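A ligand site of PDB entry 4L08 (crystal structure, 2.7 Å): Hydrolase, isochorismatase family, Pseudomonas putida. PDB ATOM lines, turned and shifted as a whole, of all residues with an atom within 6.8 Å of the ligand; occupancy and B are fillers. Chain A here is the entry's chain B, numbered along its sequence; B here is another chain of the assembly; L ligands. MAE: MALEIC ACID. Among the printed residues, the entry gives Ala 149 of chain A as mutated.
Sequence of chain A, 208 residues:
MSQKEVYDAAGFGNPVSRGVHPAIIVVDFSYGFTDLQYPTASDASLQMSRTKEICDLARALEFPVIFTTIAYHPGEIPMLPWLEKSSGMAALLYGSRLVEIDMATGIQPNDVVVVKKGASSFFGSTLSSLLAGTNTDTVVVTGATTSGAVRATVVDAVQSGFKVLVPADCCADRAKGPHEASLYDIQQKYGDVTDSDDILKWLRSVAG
The side-chain carboxylate of Asp 28 lies within salt-bridge range of the side-chain amino group of Lys 116 (2.7 Å).
O of Lys 189 of chain B is in hydrogen-bond range of NE1 of Trp 82, 3.0 Å away.
The side-chain hydroxyl of Ser 86 lies within hydrogen-bond range of the backbone carbonyl oxygen of Lys 189 of chain B (3.1 Å).
O of Thr 145 lies within hydrogen-bond range of N of Val 150 (3.0 Å).
The side-chain hydroxyl (OG1) of Thr 145 lies within hydrogen-bond range of the backbone NH (N) of Gly 148 (3.2 Å).
NZ of Lys 189 of chain B lies within hydrogen-bond range of OG of Ser 147 (3.3 Å).
The side-chain carboxylate of Asp 28 lies within hydrogen-bond range of the backbone NH of Ile 70 (3.3 Å).
The backbone NH of Ala 144 sits at hydrogen-bond distance from the backbone carbonyl oxygen of Val 27.
OG1 of Thr 145 is in hydrogen-bond range of O3 of the ligand (3.0 Å).
The backbone NH (N) of Ala 149 sits at hydrogen-bond distance from an oxygen (O3) of the ligand, at 3.0 Å.
NZ of Lys 189 of chain B lies within salt-bridge range of O1 of the ligand, at 3.2 Å.
O1 of the ligand is in salt-bridge range of NH1 of Arg 174 (3.5 Å).
O3 of the ligand sits at hydrogen-bond distance from N of Thr 145, 2.9 Å away.
The side-chain carboxylate (OD2) of Asp 28 sits close to an oxygen (O4) of the ligand, 3.0 Å away.
An oxygen (O4) of the ligand lies close to the backbone carbonyl oxygen of Ala 144 (2.9 Å).
Phe 33 touches the ligand (CE1 to C3, 3.6 Å).
Ile 70 touches the ligand.
Trp 82 touches the ligand.
CE of Met 89 touches C2 of the ligand, 3.8 Å away.
Gly 148 touches the ligand (CA to O2, 3.3 Å).
OH of Tyr 190 of chain B touches O2 of the ligand (3.8 Å).
Hydrophobic or aromatic side chains that line the ligand: Phe 33, Ile 70, Trp 82, Met 89 and Ala 149.
Within 4 Å of the ligand: Asp 28, Phe 33, Ile 70, Trp 82, Met 89, Ala 144, Thr 145, Gly 148, Ala 149, Arg 174, Lys 189 of chain B and Tyr 190 of chain B.
The nearest printed residue that does not touch the ligand is Phe 12 of chain B (4.02 Å).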
ATOM      1  N   VAL A  27      28.738  19.316 -21.971  1.00  0.00           N
ATOM      2  CA  VAL A  27      27.766  20.410 -21.906  1.00  0.00           C
ATOM      3  C   VAL A  27      27.244  20.651 -20.491  1.00  0.00           C
ATOM      4  O   VAL A  27      26.603  19.790 -19.888  1.00  0.00           O
ATOM      5  CB  VAL A  27      26.574  20.181 -22.864  1.00  0.00           C
ATOM      6  CG1 VAL A  27      25.750  21.445 -22.992  1.00  0.00           C
ATOM      7  CG2 VAL A  27      27.068  19.764 -24.248  1.00  0.00           C
ATOM      8  N   ASP A  28      27.532  21.852 -19.978  1.00  0.00           N
ATOM      9  CA  ASP A  28      26.993  22.351 -18.707  1.00  0.00           C
ATOM     10  C   ASP A  28      27.025  21.352 -17.546  1.00  0.00           C
ATOM     11  O   ASP A  28      26.024  21.151 -16.853  1.00  0.00           O
ATOM     12  CB  ASP A  28      25.558  22.877 -18.903  1.00  0.00           C
ATOM     13  CG  ASP A  28      25.498  24.110 -19.802  1.00  0.00           C
ATOM     14  OD1 ASP A  28      26.408  24.965 -19.740  1.00  0.00           O
ATOM     15  OD2 ASP A  28      24.523  24.219 -20.576  1.00  0.00           O
ATOM     16  N   PHE A  29      28.177  20.722 -17.357  1.00  0.00           N
ATOM     17  CA  PHE A  29      28.412  19.925 -16.154  1.00  0.00           C
ATOM     18  C   PHE A  29      29.061  20.798 -15.067  1.00  0.00           C
ATOM     19  O   PHE A  29      30.048  20.413 -14.452  1.00  0.00           O
ATOM     20  CB  PHE A  29      29.278  18.703 -16.447  1.00  0.00           C
ATOM     21  CG  PHE A  29      28.496  17.442 -16.730  1.00  0.00           C
ATOM     22  CD1 PHE A  29      27.215  17.261 -16.205  1.00  0.00           C
ATOM     23  CD2 PHE A  29      29.045  16.419 -17.486  1.00  0.00           C
ATOM     24  CE1 PHE A  29      26.495  16.106 -16.445  1.00  0.00           C
ATOM     25  CE2 PHE A  29      28.343  15.255 -17.729  1.00  0.00           C
ATOM     26  CZ  PHE A  29      27.060  15.097 -17.213  1.00  0.00           C
ATOM     27  N   PHE A  33      24.251  22.678 -12.235  1.00  0.00           N
ATOM     28  CA  PHE A  33      23.455  21.606 -12.847  1.00  0.00           C
ATOM     29  C   PHE A  33      23.724  20.189 -12.299  1.00  0.00           C
ATOM     30  O   PHE A  33      23.051  19.238 -12.685  1.00  0.00           O
ATOM     31  CB  PHE A  33      23.642  21.607 -14.366  1.00  0.00           C
ATOM     32  CG  PHE A  33      23.218  22.894 -15.024  1.00  0.00           C
ATOM     33  CD1 PHE A  33      21.875  23.182 -15.219  1.00  0.00           C
ATOM     34  CD2 PHE A  33      24.167  23.811 -15.452  1.00  0.00           C
ATOM     35  CE1 PHE A  33      21.486  24.364 -15.823  1.00  0.00           C
ATOM     36  CE2 PHE A  33      23.791  24.998 -16.059  1.00  0.00           C
ATOM     37  CZ  PHE A  33      22.446  25.276 -16.243  1.00  0.00           C
ATOM     38  N   ILE A  70      27.218  27.916 -18.619  1.00  0.00           N
ATOM     39  CA  ILE A  70      26.366  29.095 -18.714  1.00  0.00           C
ATOM     40  C   ILE A  70      26.760  30.033 -17.584  1.00  0.00           C
ATOM     41  O   ILE A  70      26.811  29.620 -16.425  1.00  0.00           O
ATOM     42  CB  ILE A  70      24.865  28.728 -18.652  1.00  0.00           C
ATOM     43  CG1 ILE A  70      24.507  27.717 -19.748  1.00  0.00           C
ATOM     44  CG2 ILE A  70      24.003  29.966 -18.785  1.00  0.00           C
ATOM     45  CD1 ILE A  70      23.105  27.133 -19.646  1.00  0.00           C
ATOM     46  N   TRP A  82      15.312  34.805 -22.621  1.00  0.00           N
ATOM     47  CA  TRP A  82      15.340  33.428 -22.144  1.00  0.00           C
ATOM     48  C   TRP A  82      15.335  33.367 -20.645  1.00  0.00           C
ATOM     49  O   TRP A  82      14.783  32.437 -20.048  1.00  0.00           O
ATOM     50  CB  TRP A  82      16.543  32.680 -22.705  1.00  0.00           C
ATOM     51  CG  TRP A  82      16.529  31.203 -22.366  1.00  0.00           C
ATOM     52  CD1 TRP A  82      15.484  30.297 -22.530  1.00  0.00           C
ATOM     53  CD2 TRP A  82      17.634  30.406 -21.809  1.00  0.00           C
ATOM     54  NE1 TRP A  82      15.850  29.047 -22.126  1.00  0.00           N
ATOM     55  CE2 TRP A  82      17.117  29.037 -21.680  1.00  0.00           C
ATOM     56  CE3 TRP A  82      18.944  30.675 -21.426  1.00  0.00           C
ATOM     57  CZ2 TRP A  82      17.895  28.000 -21.176  1.00  0.00           C
ATOM     58  CZ3 TRP A  82      19.717  29.628 -20.921  1.00  0.00           C
ATOM     59  CH2 TRP A  82      19.207  28.322 -20.803  1.00  0.00           C
ATOM     60  N   SER A  86      13.067  31.151 -18.106  1.00  0.00           N
ATOM     61  CA  SER A  86      13.829  30.303 -17.200  1.00  0.00           C
ATOM     62  C   SER A  86      14.603  31.185 -16.214  1.00  0.00           C
ATOM     63  O   SER A  86      15.805  31.406 -16.382  1.00  0.00           O
ATOM     64  CB  SER A  86      14.805  29.410 -17.981  1.00  0.00           C
ATOM     65  OG  SER A  86      14.135  28.761 -19.071  1.00  0.00           O
ATOM     66  N   MET A  89      18.081  30.296 -14.214  1.00  0.00           N
ATOM     67  CA  MET A  89      19.370  30.475 -14.883  1.00  0.00           C
ATOM     68  C   MET A  89      20.052  31.803 -14.522  1.00  0.00           C
ATOM     69  O   MET A  89      21.240  31.980 -14.780  1.00  0.00           O
ATOM     70  CB  MET A  89      19.217  30.368 -16.400  1.00  0.00           C
ATOM     71  CG  MET A  89      18.479  29.119 -16.863  1.00  0.00           C
ATOM     72  SD  MET A  89      19.466  27.619 -16.664  1.00  0.00           S
ATOM     73  CE  MET A  89      18.212  26.470 -16.110  1.00  0.00           C
ATOM     74  N   LYS A 116      28.733  30.445 -22.451  1.00  0.00           N
ATOM     75  CA  LYS A 116      27.590  30.701 -23.326  1.00  0.00           C
ATOM     76  C   LYS A 116      26.441  31.301 -22.533  1.00  0.00           C
ATOM     77  O   LYS A 116      26.406  31.205 -21.304  1.00  0.00           O
ATOM     78  CB  LYS A 116      27.177  29.417 -24.044  1.00  0.00           C
ATOM     79  CG  LYS A 116      26.701  28.289 -23.138  1.00  0.00           C
ATOM     80  CD  LYS A 116      26.485  27.012 -23.927  1.00  0.00           C
ATOM     81  CE  LYS A 116      26.018  25.867 -23.044  1.00  0.00           C
ATOM     82  NZ  LYS A 116      24.596  26.020 -22.631  1.00  0.00           N
ATOM     83  N   GLY A 118      23.021  30.993 -23.815  1.00  0.00           N
ATOM     84  CA  GLY A 118      21.815  30.257 -24.172  1.00  0.00           C
ATOM     85  C   GLY A 118      21.930  28.766 -23.905  1.00  0.00           C
ATOM     86  O   GLY A 118      22.870  28.319 -23.243  1.00  0.00           O
ATOM     87  N   ALA A 119      20.963  28.012 -24.412  1.00  0.00           N
ATOM     88  CA  ALA A 119      20.917  26.565 -24.219  1.00  0.00           C
ATOM     89  C   ALA A 119      21.946  25.820 -25.077  1.00  0.00           C
ATOM     90  O   ALA A 119      22.686  24.993 -24.562  1.00  0.00           O
ATOM     91  CB  ALA A 119      19.517  26.045 -24.501  1.00  0.00           C
ATOM     92  N   ALA A 144      24.463  17.898 -19.398  1.00  0.00           N
ATOM     93  CA  ALA A 144      23.158  18.159 -18.820  1.00  0.00           C
ATOM     94  C   ALA A 144      22.638  19.528 -19.289  1.00  0.00           C
ATOM     95  O   ALA A 144      23.423  20.456 -19.448  1.00  0.00           O
ATOM     96  CB  ALA A 144      23.242  18.110 -17.305  1.00  0.00           C
ATOM     97  N   THR A 145      21.336  19.646 -19.534  1.00  0.00           N
ATOM     98  CA  THR A 145      20.389  18.538 -19.443  1.00  0.00           C
ATOM     99  C   THR A 145      20.071  18.006 -20.831  1.00  0.00           C
ATOM    100  O   THR A 145      20.168  18.737 -21.825  1.00  0.00           O
ATOM    101  CB  THR A 145      19.081  18.944 -18.730  1.00  0.00           C
ATOM    102  OG1 THR A 145      18.402  19.949 -19.494  1.00  0.00           O
ATOM    103  CG2 THR A 145      19.359  19.486 -17.336  1.00  0.00           C
ATOM    104  N   THR A 146      19.696  16.732 -20.896  1.00  0.00           N
ATOM    105  CA  THR A 146      19.476  16.045 -22.170  1.00  0.00           C
ATOM    106  C   THR A 146      18.343  16.636 -23.000  1.00  0.00           C
ATOM    107  O   THR A 146      18.438  16.714 -24.219  1.00  0.00           O
ATOM    108  CB  THR A 146      19.356  14.510 -22.007  1.00  0.00           C
ATOM    109  OG1 THR A 146      18.246  14.003 -22.771  1.00  0.00           O
ATOM    110  CG2 THR A 146      19.160  14.139 -20.554  1.00  0.00           C
ATOM    111  N   SER A 147      17.267  17.067 -22.334  1.00  0.00           N
ATOM    112  CA  SER A 147      16.163  17.732 -23.016  1.00  0.00           C
ATOM    113  C   SER A 147      16.421  19.230 -23.191  1.00  0.00           C
ATOM    114  O   SER A 147      15.659  19.922 -23.887  1.00  0.00           O
ATOM    115  CB  SER A 147      14.837  17.485 -22.291  1.00  0.00           C
ATOM    116  OG  SER A 147      14.831  18.063 -21.003  1.00  0.00           O
ATOM    117  N   GLY A 148      17.489  19.726 -22.573  1.00  0.00           N
ATOM    118  CA  GLY A 148      17.822  21.136 -22.640  1.00  0.00           C
ATOM    119  C   GLY A 148      19.031  21.423 -23.507  1.00  0.00           C
ATOM    120  O   GLY A 148      18.951  21.386 -24.741  1.00  0.00           O
ATOM    121  N   ALA A 149      20.152  21.725 -22.860  1.00  0.00           N
ATOM    122  CA  ALA A 149      21.375  22.129 -23.535  1.00  0.00           C
ATOM    123  C   ALA A 149      21.998  21.049 -24.415  1.00  0.00           C
ATOM    124  O   ALA A 149      22.588  21.359 -25.445  1.00  0.00           O
ATOM    125  CB  ALA A 149      22.398  22.627 -22.524  1.00  0.00           C
ATOM    126  N   VAL A 150      21.867  19.782 -24.002  1.00  0.00           N
ATOM    127  CA  VAL A 150      22.443  18.688 -24.783  1.00  0.00           C
ATOM    128  C   VAL A 150      21.791  18.607 -26.159  1.00  0.00           C
ATOM    129  O   VAL A 150      22.486  18.719 -27.170  1.00  0.00           O
ATOM    130  CB  VAL A 150      22.369  17.334 -24.037  1.00  0.00           C
ATOM    131  CG1 VAL A 150      22.878  16.211 -24.920  1.00  0.00           C
ATOM    132  CG2 VAL A 150      23.190  17.401 -22.759  1.00  0.00           C
ATOM    133  N   ASP A 173      19.264  14.397 -16.839  1.00  0.00           N
ATOM    134  CA  ASP A 173      18.145  15.336 -16.844  1.00  0.00           C
ATOM    135  C   ASP A 173      17.447  15.304 -15.487  1.00  0.00           C
ATOM    136  O   ASP A 173      17.734  14.423 -14.659  1.00  0.00           O
ATOM    137  CB  ASP A 173      17.152  14.996 -17.958  1.00  0.00           C
ATOM    138  CG  ASP A 173      16.495  16.235 -18.569  1.00  0.00           C
ATOM    139  OD1 ASP A 173      16.292  17.259 -17.859  1.00  0.00           O
ATOM    140  OD2 ASP A 173      16.179  16.197 -19.775  1.00  0.00           O
ATOM    141  N   ARG A 174      16.551  16.246 -15.255  1.00  0.00           N
ATOM    142  CA  ARG A 174      15.825  16.323 -13.993  1.00  0.00           C
ATOM    143  C   ARG A 174      14.518  15.516 -13.992  1.00  0.00           C
ATOM    144  O   ARG A 174      13.876  15.367 -12.960  1.00  0.00           O
ATOM    145  CB  ARG A 174      15.585  17.786 -13.573  1.00  0.00           C
ATOM    146  CG  ARG A 174      15.016  18.692 -14.660  1.00  0.00           C
ATOM    147  CD  ARG A 174      14.861  20.126 -14.183  1.00  0.00           C
ATOM    148  NE  ARG A 174      16.140  20.843 -14.071  1.00  0.00           N
ATOM    149  CZ  ARG A 174      16.734  21.501 -15.065  1.00  0.00           C
ATOM    150  NH1 ARG A 174      16.188  21.546 -16.273  1.00  0.00           N
ATOM    151  NH2 ARG A 174      17.893  22.105 -14.854  1.00  0.00           N
ATOM    152  N   TYR B   7      10.524  21.327 -11.724  1.00  0.00           N
ATOM    153  CA  TYR B   7      10.588  22.341 -12.768  1.00  0.00           C
ATOM    154  C   TYR B   7      10.274  23.746 -12.266  1.00  0.00           C
ATOM    155  O   TYR B   7      10.777  24.737 -12.804  1.00  0.00           O
ATOM    156  CB  TYR B   7       9.677  21.956 -13.936  1.00  0.00           C
ATOM    157  CG  TYR B   7      10.368  21.102 -14.975  1.00  0.00           C
ATOM    158  CD1 TYR B   7      10.873  21.670 -16.149  1.00  0.00           C
ATOM    159  CD2 TYR B   7      10.516  19.724 -14.791  1.00  0.00           C
ATOM    160  CE1 TYR B   7      11.514  20.891 -17.107  1.00  0.00           C
ATOM    161  CE2 TYR B   7      11.143  18.940 -15.747  1.00  0.00           C
ATOM    162  CZ  TYR B   7      11.639  19.526 -16.899  1.00  0.00           C
ATOM    163  OH  TYR B   7      12.271  18.752 -17.856  1.00  0.00           O
ATOM    164  N   PHE B  12      11.504  27.441 -13.964  1.00  0.00           N
ATOM    165  CA  PHE B  12      10.845  27.323 -15.269  1.00  0.00           C
ATOM    166  C   PHE B  12       9.353  27.648 -15.186  1.00  0.00           C
ATOM    167  O   PHE B  12       8.785  27.735 -14.101  1.00  0.00           O
ATOM    168  CB  PHE B  12      11.035  25.921 -15.842  1.00  0.00           C
ATOM    169  CG  PHE B  12      12.472  25.565 -16.150  1.00  0.00           C
ATOM    170  CD1 PHE B  12      13.174  26.235 -17.151  1.00  0.00           C
ATOM    171  CD2 PHE B  12      13.112  24.553 -15.461  1.00  0.00           C
ATOM    172  CE1 PHE B  12      14.484  25.911 -17.438  1.00  0.00           C
ATOM    173  CE2 PHE B  12      14.432  24.224 -15.739  1.00  0.00           C
ATOM    174  CZ  PHE B  12      15.118  24.903 -16.728  1.00  0.00           C
ATOM    175  N   LYS B 189      10.516  26.106 -20.871  1.00  0.00           N
ATOM    176  CA  LYS B 189      11.860  26.657 -21.076  1.00  0.00           C
ATOM    177  C   LYS B 189      11.988  27.835 -22.046  1.00  0.00           C
ATOM    178  O   LYS B 189      12.843  28.693 -21.843  1.00  0.00           O
ATOM    179  CB  LYS B 189      12.819  25.548 -21.503  1.00  0.00           C
ATOM    180  CG  LYS B 189      13.022  24.441 -20.483  1.00  0.00           C
ATOM    181  CD  LYS B 189      13.910  23.348 -21.040  1.00  0.00           C
ATOM    182  CE  LYS B 189      14.166  22.272 -19.998  1.00  0.00           C
ATOM    183  NZ  LYS B 189      15.159  21.266 -20.469  1.00  0.00           N
ATOM    184  N   TYR B 190      11.168  27.871 -23.090  1.00  0.00           N
ATOM    185  CA  TYR B 190      11.460  28.741 -24.234  1.00  0.00           C
ATOM    186  C   TYR B 190      10.409  29.802 -24.603  1.00  0.00           C
ATOM    187  O   TYR B 190      10.770  30.922 -24.964  1.00  0.00           O
ATOM    188  CB  TYR B 190      11.817  27.899 -25.462  1.00  0.00           C
ATOM    189  CG  TYR B 190      12.906  26.879 -25.189  1.00  0.00           C
ATOM    190  CD1 TYR B 190      14.210  27.279 -24.905  1.00  0.00           C
ATOM    191  CD2 TYR B 190      12.626  25.514 -25.221  1.00  0.00           C
ATOM    192  CE1 TYR B 190      15.208  26.350 -24.646  1.00  0.00           C
ATOM    193  CE2 TYR B 190      13.619  24.576 -24.962  1.00  0.00           C
ATOM    194  CZ  TYR B 190      14.913  25.003 -24.685  1.00  0.00           C
ATOM    195  OH  TYR B 190      15.901  24.079 -24.425  1.00  0.00           O
HETATM  196  C1  MAE L   1      18.016  23.839 -19.896  1.00  0.00           C
HETATM  197  O1  MAE L   1      17.634  22.900 -19.143  1.00  0.00           O
HETATM  198  O2  MAE L   1      17.586  24.007 -21.060  1.00  0.00           O
HETATM  199  C2  MAE L   1      19.013  24.802 -19.379  1.00  0.00           C
HETATM  200  C3  MAE L   1      20.305  24.529 -19.186  1.00  0.00           C
HETATM  201  C4  MAE L   1      20.949  23.219 -19.445  1.00  0.00           C
HETATM  202  O3  MAE L   1      20.314  22.274 -19.959  1.00  0.00           O
HETATM  203  O4  MAE L   1      22.153  23.087 -19.134  1.00  0.00           O
